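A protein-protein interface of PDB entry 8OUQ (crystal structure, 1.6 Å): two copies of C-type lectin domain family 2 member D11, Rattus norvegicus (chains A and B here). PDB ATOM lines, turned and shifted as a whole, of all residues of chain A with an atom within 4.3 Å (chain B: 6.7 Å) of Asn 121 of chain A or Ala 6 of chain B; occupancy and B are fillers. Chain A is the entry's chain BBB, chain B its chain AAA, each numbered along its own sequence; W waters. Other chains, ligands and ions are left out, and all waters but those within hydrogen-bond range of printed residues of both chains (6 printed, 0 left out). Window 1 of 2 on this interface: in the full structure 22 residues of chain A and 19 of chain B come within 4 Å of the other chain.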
ATOM      1  N   TYR A   4      -9.428 -31.579 -12.601  1.00  0.00           N
ATOM      2  CA  TYR A   4      -8.170 -31.334 -13.343  1.00  0.00           C
ATOM      3  C   TYR A   4      -8.240 -29.915 -13.856  1.00  0.00           C
ATOM      4  O   TYR A   4      -9.277 -29.464 -14.386  1.00  0.00           O
ATOM      5  CB  TYR A   4      -7.980 -32.345 -14.470  1.00  0.00           C
ATOM      6  CG  TYR A   4      -7.636 -33.727 -13.982  1.00  0.00           C
ATOM      7  CD1 TYR A   4      -6.420 -33.986 -13.375  1.00  0.00           C
ATOM      8  CD2 TYR A   4      -8.506 -34.794 -14.173  1.00  0.00           C
ATOM      9  CE1 TYR A   4      -6.101 -35.248 -12.912  1.00  0.00           C
ATOM     10  CE2 TYR A   4      -8.192 -36.070 -13.732  1.00  0.00           C
ATOM     11  CZ  TYR A   4      -6.977 -36.299 -13.112  1.00  0.00           C
ATOM     12  OH  TYR A   4      -6.629 -37.537 -12.650  1.00  0.00           O
ATOM     13  N   ALA A   5      -7.162 -29.180 -13.678  1.00  0.00           N
ATOM     14  CA  ALA A   5      -7.076 -27.814 -14.191  1.00  0.00           C
ATOM     15  C   ALA A   5      -5.614 -27.480 -14.458  1.00  0.00           C
ATOM     16  O   ALA A   5      -4.787 -27.703 -13.569  1.00  0.00           O
ATOM     17  CB  ALA A   5      -7.693 -26.858 -13.228  1.00  0.00           C
ATOM     18  N   CYS A   7      -2.170 -25.532 -14.728  1.00  0.00           N
ATOM     19  CA  CYS A   7      -1.522 -24.367 -14.088  1.00  0.00           C
ATOM     20  C   CYS A   7      -1.508 -23.211 -15.087  1.00  0.00           C
ATOM     21  O   CYS A   7      -1.466 -23.401 -16.304  1.00  0.00           O
ATOM     22  CB  CYS A   7      -0.102 -24.704 -13.626  1.00  0.00           C
ATOM     23  SG  CYS A   7      -0.093 -25.953 -12.318  1.00  0.00           S
ATOM     24  N   GLY A  13       2.702 -27.951 -13.486  1.00  0.00           N
ATOM     25  CA  GLY A  13       1.868 -28.704 -12.556  1.00  0.00           C
ATOM     26  C   GLY A  13       2.401 -30.043 -12.211  1.00  0.00           C
ATOM     27  O   GLY A  13       2.753 -30.874 -13.115  1.00  0.00           O
ATOM     28  N   GLY A  15       1.412 -33.066  -9.227  1.00  0.00           N
ATOM     29  CA  GLY A  15       0.450 -33.381  -8.155  1.00  0.00           C
ATOM     30  C   GLY A  15      -0.556 -32.249  -8.030  1.00  0.00           C
ATOM     31  O   GLY A  15      -1.008 -31.743  -9.058  1.00  0.00           O
ATOM     32  N   ASN A  16      -0.818 -31.793  -6.815  1.00  0.00           N
ATOM     33  CA  ASN A  16      -1.842 -30.750  -6.597  1.00  0.00           C
ATOM     34  C   ASN A  16      -1.198 -29.366  -6.535  1.00  0.00           C
ATOM     35  O   ASN A  16      -1.858 -28.434  -6.060  1.00  0.00           O
ATOM     36  CB  ASN A  16      -2.660 -31.085  -5.362  1.00  0.00           C
ATOM     37  CG  ASN A  16      -1.906 -30.978  -4.061  1.00  0.00           C
ATOM     38  OD1 ASN A  16      -0.703 -30.671  -3.990  1.00  0.00           O
ATOM     39  ND2 ASN A  16      -2.644 -31.195  -2.985  1.00  0.00           N
ATOM     40  N   LYS A  17       0.050 -29.221  -7.002  1.00  0.00           N
ATOM     41  CA  LYS A  17       0.777 -27.923  -6.948  1.00  0.00           C
ATOM     42  C   LYS A  17       1.092 -27.370  -8.336  1.00  0.00           C
ATOM     43  O   LYS A  17       1.141 -28.130  -9.327  1.00  0.00           O
ATOM     44  CB  LYS A  17       2.139 -28.094  -6.269  1.00  0.00           C
ATOM     45  CG  LYS A  17       2.096 -28.687  -4.873  1.00  0.00           C
ATOM     46  CD  LYS A  17       1.969 -27.638  -3.836  1.00  0.00           C
ATOM     47  CE  LYS A  17       2.064 -28.150  -2.412  1.00  0.00           C
ATOM     48  NZ  LYS A  17       3.456 -28.399  -1.964  1.00  0.00           N
ATOM     49  N   CYS A  18       1.394 -26.068  -8.359  1.00  0.00           N
ATOM     50  CA  CYS A  18       1.914 -25.315  -9.521  1.00  0.00           C
ATOM     51  C   CYS A  18       3.251 -24.715  -9.081  1.00  0.00           C
ATOM     52  O   CYS A  18       3.307 -24.182  -7.951  1.00  0.00           O
ATOM     53  CB  CYS A  18       0.940 -24.240  -9.999  1.00  0.00           C
ATOM     54  SG  CYS A  18      -0.660 -24.926 -10.584  1.00  0.00           S
ATOM     55  N   ARG A 119       2.488 -22.994  -5.340  1.00  0.00           N
ATOM     56  CA  ARG A 119       1.176 -22.737  -4.696  1.00  0.00           C
ATOM     57  C   ARG A 119       0.267 -23.914  -4.987  1.00  0.00           C
ATOM     58  O   ARG A 119       0.507 -24.684  -5.956  1.00  0.00           O
ATOM     59  CB  ARG A 119       0.506 -21.436  -5.124  1.00  0.00           C
ATOM     60  CG  ARG A 119       0.474 -21.240  -6.613  1.00  0.00           C
ATOM     61  CD  ARG A 119      -0.020 -19.867  -7.029  1.00  0.00           C
ATOM     62  NE  ARG A 119      -0.151 -19.938  -8.467  1.00  0.00           N
ATOM     63  CZ  ARG A 119      -0.107 -18.920  -9.316  1.00  0.00           C
ATOM     64  NH1 ARG A 119       0.116 -17.678  -8.911  1.00  0.00           N
ATOM     65  NH2 ARG A 119      -0.244 -19.185 -10.604  1.00  0.00           N
ATOM     66  N   LEU A 120      -0.716 -24.100  -4.123  1.00  0.00           N
ATOM     67  CA  LEU A 120      -1.677 -25.199  -4.402  1.00  0.00           C
ATOM     68  C   LEU A 120      -2.431 -24.799  -5.677  1.00  0.00           C
ATOM     69  O   LEU A 120      -2.791 -23.613  -5.831  1.00  0.00           O
ATOM     70  CB  LEU A 120      -2.618 -25.394  -3.216  1.00  0.00           C
ATOM     71  CG  LEU A 120      -1.996 -26.114  -2.034  1.00  0.00           C
ATOM     72  CD1 LEU A 120      -2.835 -25.893  -0.764  1.00  0.00           C
ATOM     73  CD2 LEU A 120      -1.824 -27.581  -2.343  1.00  0.00           C
ATOM     74  N   ASN A 121      -2.730 -25.763  -6.528  1.00  0.00           N
ATOM     75  CA  ASN A 121      -3.501 -25.521  -7.764  1.00  0.00           C
ATOM     76  C   ASN A 121      -4.920 -25.108  -7.330  1.00  0.00           C
ATOM     77  O   ASN A 121      -5.582 -25.933  -6.719  1.00  0.00           O
ATOM     78  CB  ASN A 121      -3.453 -26.773  -8.619  1.00  0.00           C
ATOM     79  CG  ASN A 121      -4.120 -26.632  -9.967  1.00  0.00           C
ATOM     80  OD1 ASN A 121      -5.014 -25.800 -10.131  1.00  0.00           O
ATOM     81  ND2 ASN A 121      -3.673 -27.428 -10.927  1.00  0.00           N
ATOM     82  N   SER A 122      -5.390 -23.937  -7.737  1.00  0.00           N
ATOM     83  CA  SER A 122      -6.696 -23.392  -7.288  1.00  0.00           C
ATOM     84  C   SER A 122      -7.817 -23.751  -8.264  1.00  0.00           C
ATOM     85  O   SER A 122      -8.965 -23.311  -8.015  1.00  0.00           O
ATOM     86  CB  SER A 122      -6.613 -21.912  -7.119  1.00  0.00           C
ATOM     87  OG  SER A 122      -6.644 -21.271  -8.386  1.00  0.00           O
ATOM     88  N   GLY A 123      -7.499 -24.439  -9.363  1.00  0.00           N
ATOM     89  CA  GLY A 123      -8.430 -24.743 -10.468  1.00  0.00           C
ATOM     90  C   GLY A 123      -8.926 -23.523 -11.224  1.00  0.00           C
ATOM     91  O   GLY A 123     -10.034 -23.623 -11.821  1.00  0.00           O
ATOM     92  N   THR B   2      -5.899 -34.249  -2.669  1.00  0.00           N
ATOM     93  CA  THR B   2      -6.980 -33.268  -2.431  1.00  0.00           C
ATOM     94  C   THR B   2      -6.744 -32.043  -3.305  1.00  0.00           C
ATOM     95  O   THR B   2      -5.561 -31.721  -3.593  1.00  0.00           O
ATOM     96  CB  THR B   2      -7.037 -32.861  -0.958  1.00  0.00           C
ATOM     97  OG1 THR B   2      -5.763 -32.263  -0.704  1.00  0.00           O
ATOM     98  CG2 THR B   2      -7.292 -34.050  -0.054  1.00  0.00           C
ATOM     99  N   GLY B   3      -7.834 -31.382  -3.682  1.00  0.00           N
ATOM    100  CA  GLY B   3      -7.813 -30.154  -4.489  1.00  0.00           C
ATOM    101  C   GLY B   3      -7.605 -30.431  -5.955  1.00  0.00           C
ATOM    102  O   GLY B   3      -8.049 -31.459  -6.453  1.00  0.00           O
ATOM    103  N   TYR B   4      -6.985 -29.504  -6.672  1.00  0.00           N
ATOM    104  CA  TYR B   4      -6.915 -29.625  -8.145  1.00  0.00           C
ATOM    105  C   TYR B   4      -5.535 -30.159  -8.528  1.00  0.00           C
ATOM    106  O   TYR B   4      -4.569 -29.858  -7.826  1.00  0.00           O
ATOM    107  CB  TYR B   4      -7.177 -28.293  -8.828  1.00  0.00           C
ATOM    108  CG  TYR B   4      -8.619 -27.842  -8.779  1.00  0.00           C
ATOM    109  CD1 TYR B   4      -9.093 -27.064  -7.728  1.00  0.00           C
ATOM    110  CD2 TYR B   4      -9.479 -28.159  -9.803  1.00  0.00           C
ATOM    111  CE1 TYR B   4     -10.402 -26.592  -7.719  1.00  0.00           C
ATOM    112  CE2 TYR B   4     -10.809 -27.745  -9.776  1.00  0.00           C
ATOM    113  CZ  TYR B   4     -11.251 -26.928  -8.749  1.00  0.00           C
ATOM    114  OH  TYR B   4     -12.530 -26.452  -8.770  1.00  0.00           O
ATOM    115  N   ALA B   5      -5.482 -30.882  -9.639  1.00  0.00           N
ATOM    116  CA  ALA B   5      -4.218 -31.287 -10.307  1.00  0.00           C
ATOM    117  C   ALA B   5      -4.263 -30.916 -11.791  1.00  0.00           C
ATOM    118  O   ALA B   5      -5.329 -30.919 -12.403  1.00  0.00           O
ATOM    119  CB  ALA B   5      -3.995 -32.746 -10.143  1.00  0.00           C
ATOM    120  N   ALA B   6      -3.123 -30.557 -12.370  1.00  0.00           N
ATOM    121  CA  ALA B   6      -3.011 -30.353 -13.823  1.00  0.00           C
ATOM    122  C   ALA B   6      -3.200 -31.711 -14.476  1.00  0.00           C
ATOM    123  O   ALA B   6      -3.937 -31.811 -15.545  1.00  0.00           O
ATOM    124  CB  ALA B   6      -1.666 -29.723 -14.200  1.00  0.00           C
ATOM    125  N   CYS B   7      -2.555 -32.720 -13.889  1.00  0.00           N
ATOM    126  CA  CYS B   7      -2.353 -34.035 -14.550  1.00  0.00           C
ATOM    127  C   CYS B   7      -2.502 -35.167 -13.543  1.00  0.00           C
ATOM    128  O   CYS B   7      -2.292 -35.003 -12.359  1.00  0.00           O
ATOM    129  CB  CYS B   7      -0.954 -34.056 -15.177  1.00  0.00           C
ATOM    130  SG  CYS B   7      -0.728 -32.760 -16.405  1.00  0.00           S
ATOM    131  N   PRO B   8      -2.686 -36.405 -14.034  1.00  0.00           N
ATOM    132  CA  PRO B   8      -2.605 -37.569 -13.157  1.00  0.00           C
ATOM    133  C   PRO B   8      -1.216 -37.798 -12.566  1.00  0.00           C
ATOM    134  O   PRO B   8      -0.207 -37.201 -12.994  1.00  0.00           O
ATOM    135  CB  PRO B   8      -2.924 -38.728 -14.117  1.00  0.00           C
ATOM    136  CG  PRO B   8      -3.663 -38.106 -15.246  1.00  0.00           C
ATOM    137  CD  PRO B   8      -3.013 -36.753 -15.420  1.00  0.00           C
ATOM    138  N   ILE B  12       3.349 -34.510 -15.826  1.00  0.00           N
ATOM    139  CA  ILE B  12       3.742 -33.105 -15.540  1.00  0.00           C
ATOM    140  C   ILE B  12       2.953 -32.167 -16.452  1.00  0.00           C
ATOM    141  O   ILE B  12       2.929 -32.410 -17.679  1.00  0.00           O
ATOM    142  CB  ILE B  12       5.271 -32.925 -15.659  1.00  0.00           C
ATOM    143  CG1 ILE B  12       6.051 -33.847 -14.732  1.00  0.00           C
ATOM    144  CG2 ILE B  12       5.702 -31.513 -15.413  1.00  0.00           C
ATOM    145  CD1 ILE B  12       7.515 -33.980 -15.132  1.00  0.00           C
ATOM    146  N   GLY B  13       2.296 -31.115 -15.878  1.00  0.00           N
ATOM    147  CA  GLY B  13       1.455 -30.230 -16.693  1.00  0.00           C
ATOM    148  C   GLY B  13       2.139 -28.982 -17.142  1.00  0.00           C
ATOM    149  O   GLY B  13       2.793 -28.279 -16.317  1.00  0.00           O
ATOM    150  N   VAL B  14       2.099 -28.755 -18.451  1.00  0.00           N
ATOM    151  CA  VAL B  14       2.662 -27.542 -19.083  1.00  0.00           C
ATOM    152  C   VAL B  14       1.623 -27.051 -20.083  1.00  0.00           C
ATOM    153  O   VAL B  14       1.323 -27.850 -20.983  1.00  0.00           O
ATOM    154  CB  VAL B  14       4.006 -27.846 -19.771  1.00  0.00           C
ATOM    155  CG1 VAL B  14       4.519 -26.633 -20.525  1.00  0.00           C
ATOM    156  CG2 VAL B  14       5.008 -28.358 -18.770  1.00  0.00           C
ATOM    157  N   GLY B  15       1.112 -25.833 -19.894  1.00  0.00           N
ATOM    158  CA  GLY B  15       0.057 -25.278 -20.752  1.00  0.00           C
ATOM    159  C   GLY B  15      -1.102 -26.219 -20.767  1.00  0.00           C
ATOM    160  O   GLY B  15      -1.542 -26.611 -19.679  1.00  0.00           O
ATOM    161  N   LYS B  17      -1.065 -29.324 -21.915  1.00  0.00           N
ATOM    162  CA  LYS B  17      -0.548 -30.703 -22.078  1.00  0.00           C
ATOM    163  C   LYS B  17      -0.177 -31.319 -20.737  1.00  0.00           C
ATOM    164  O   LYS B  17       0.150 -30.594 -19.780  1.00  0.00           O
ATOM    165  CB  LYS B  17       0.736 -30.726 -22.926  1.00  0.00           C
ATOM    166  CG  LYS B  17       0.549 -30.158 -24.314  1.00  0.00           C
ATOM    167  CD  LYS B  17      -0.079 -31.188 -25.191  1.00  0.00           C
ATOM    168  CE  LYS B  17      -0.160 -30.777 -26.640  1.00  0.00           C
ATOM    169  NZ  LYS B  17       1.184 -30.724 -27.229  1.00  0.00           N
ATOM    170  N   CYS B  18      -0.193 -32.652 -20.707  1.00  0.00           N
ATOM    171  CA  CYS B  18       0.386 -33.476 -19.627  1.00  0.00           C
ATOM    172  C   CYS B  18       1.479 -34.317 -20.274  1.00  0.00           C
ATOM    173  O   CYS B  18       1.236 -34.818 -21.376  1.00  0.00           O
ATOM    174  CB  CYS B  18      -0.662 -34.368 -18.974  1.00  0.00           C
ATOM    175  SG  CYS B  18      -1.867 -33.371 -18.046  1.00  0.00           S
ATOM    176  N   ASN B 121      -4.733 -31.917 -22.035  1.00  0.00           N
ATOM    177  CA  ASN B 121      -5.394 -31.687 -20.714  1.00  0.00           C
ATOM    178  C   ASN B 121      -4.327 -31.308 -19.690  1.00  0.00           C
ATOM    179  O   ASN B 121      -4.308 -30.124 -19.335  1.00  0.00           O
ATOM    180  CB  ASN B 121      -6.267 -32.848 -20.229  1.00  0.00           C
ATOM    181  CG  ASN B 121      -7.613 -32.899 -20.926  1.00  0.00           C
ATOM    182  OD1 ASN B 121      -7.860 -32.160 -21.882  1.00  0.00           O
ATOM    183  ND2 ASN B 121      -8.486 -33.779 -20.463  1.00  0.00           N
HETATM  184  O   HOH W   1      -0.571 -32.114 -11.860  1.00  0.00           O
HETATM  185  O   HOH W   2      -0.339 -27.113 -16.233  1.00  0.00           O
HETATM  186  O   HOH W   3       0.919 -34.642 -11.583  1.00  0.00           O
HETATM  187  O   HOH W   4      -1.267 -29.157 -10.310  1.00  0.00           O
HETATM  188  O   HOH W   5       0.947 -24.888 -17.088  1.00  0.00           O
HETATM  189  O   HOH W   6      -4.768 -27.948  -5.244  1.00  0.00           O
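The backbone carbonyl oxygen of Thr 2 of chain B lies within hydrogen-bond range of the side-chain amide nitrogen of Asn 16 of chain A (3.0 Å).
N of Ala 5 of chain A is in hydrogen-bond range of O of Ala 5 of chain B, 2.8 Å away.
The side-chain amide nitrogen of Asn 121 of chain A lies close to the backbone NH of Ala 6 of chain B (3.5 Å).
N of Gly 13 of chain B lies within hydrogen-bond range of O of Gly 13 of chain A, at 2.8 Å.
The side-chain sulfur of Cys 7 of chain B sits close to the backbone NH of Gly 13 of chain B, 3.5 Å away.
The side-chain sulfur (SG) of Cys 7 of chain B forms a disulfide with the side-chain sulfur (SG) of Cys 18 of chain B (2.1 Å).
The backbone carbonyl oxygen (O) of Ala 5 of chain A sits at hydrogen-bond distance from the side-chain amide nitrogen (ND2) of Asn 121 of chain A, 2.9 Å away.
The side-chain sulfur (SG) of Cys 7 of chain A sits close to the backbone NH (N) of Gly 13 of chain A.
N of Asn 121 of chain A lies within hydrogen-bond range of O of Asn 16 of chain A (2.8 Å).
The side-chain amide oxygen (OD1) of Asn 121 of chain A sits at hydrogen-bond distance from the backbone NH (N) of Gly 123 of chain A (2.9 Å).
CA of Tyr 4 of chain A touches O of Ala 5 of chain B, 3.0 Å away.
CE1 of Tyr 4 of chain A touches C of Cys 7 of chain B, at 3.7 Å.
CE1 of Tyr 4 of chain A touches N of Pro 8 of chain B, at 3.8 Å.
CA of Ala 6 of chain B touches O of Ala 5 of chain A (3.2 Å).
O of Gly 15 of chain A touches CB of Ala 5 of chain B, at 3.3 Å.
Asn 16 of chain A touches Tyr 4 of chain B.
Asn 121 of chain A touches Tyr 4 of chain B (CB to O, 3.4 Å).
Asn 121 of chain A touches Ala 5 of chain B.
CD1 of Tyr 4 of chain B touches C of Ser 122 of chain A, at 3.6 Å.
Gly 123 of chain A touches Tyr 4 of chain B.
Of chain B, only Tyr 4, Ala 5 and Ala 6 come within 4 Å of Asn 121 of chain A.
Of the printed residues of chain A, Tyr 4 of chain B touches Asn 16, Asn 121, Ser 122 and Gly 123.
Of the printed residues of chain B, Ala 5 of chain A touches Ala 5 and Ala 6.
The nearest residue of chain B that does not touch Asn 121 of chain A is Gly 3 of chain B (5.0 Å).
The nearest residue of chain A that does not touch Ala 6 of chain B is Gly 13 of chain A (4.03 Å).
The nearest printed residue of chain A that does not touch Thr 2 of chain B is Leu 120 of chain A (5.7 Å).
Hydrophobic or aromatic side chains of chain B that line the printed part of chain A: Tyr 4, Ala 5, Ala 6, Pro 8 and Ile 12.
Among the printed residues, no Asp or Glu carboxylate lies within 4 Å of a Lys or Arg side-chain nitrogen of the other chain.
Tyr 4 of chain A touches Cys 7 of chain B, but with the chains exchanged Cys 7 of chain A does not touch Tyr 4 of chain B (7.4 Å).
Ala 5 of chain A touches its own counterpart, Ala 5 of chain B.
Gly 13 of chain A touches its own counterpart, Gly 13 of chain B.
Asn 121 of chain A touches Ala 5 of chain B, but with the chains exchanged Ala 5 of chain A does not touch Asn 121 of chain B (5.7 Å).
Of the 16 pairs that touch across the chains among the printed residues, 2 have their exchanged pair printed and touching as well.
Water W6 lies within hydrogen-bond range of O of Asn 121 of chain A (2.6 Å), O of Asn 16 of chain A (3.1 Å) and N of Tyr 4 of chain B (3.1 Å).
Water W4 lies within hydrogen-bond range of the backbone carbonyl oxygen (O) of Lys 17 of chain A (2.8 Å), the backbone carbonyl oxygen (O) of Gly 15 of chain A (2.9 Å), the side-chain amide nitrogen (ND2) of Asn 121 of chain A (3.0 Å) and the backbone NH (N) of Ala 6 of chain B (3.1 Å).
Water W2 lies within hydrogen-bond range of the backbone NH of Cys 7 of chain A (2.8 Å) and the backbone carbonyl oxygen of Gly 13 of chain B (3.3 Å).
Water W1 lies within hydrogen-bond range of the backbone carbonyl oxygen (O) of Gly 15 of chain A (2.9 Å), the backbone NH (N) of Cys 7 of chain B (2.9 Å) and the backbone NH (N) of Ala 6 of chain B (3.0 Å).
Water W3 lies within hydrogen-bond range of N of Gly 15 of chain A (2.9 Å), O of Pro 8 of chain B (3.1 Å) and O of Cys 7 of chain B (3.3 Å).
Water W5 lies within hydrogen-bond range of the backbone carbonyl oxygen of Cys 7 of chain A (2.9 Å) and the backbone NH of Gly 15 of chain B (3.0 Å).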
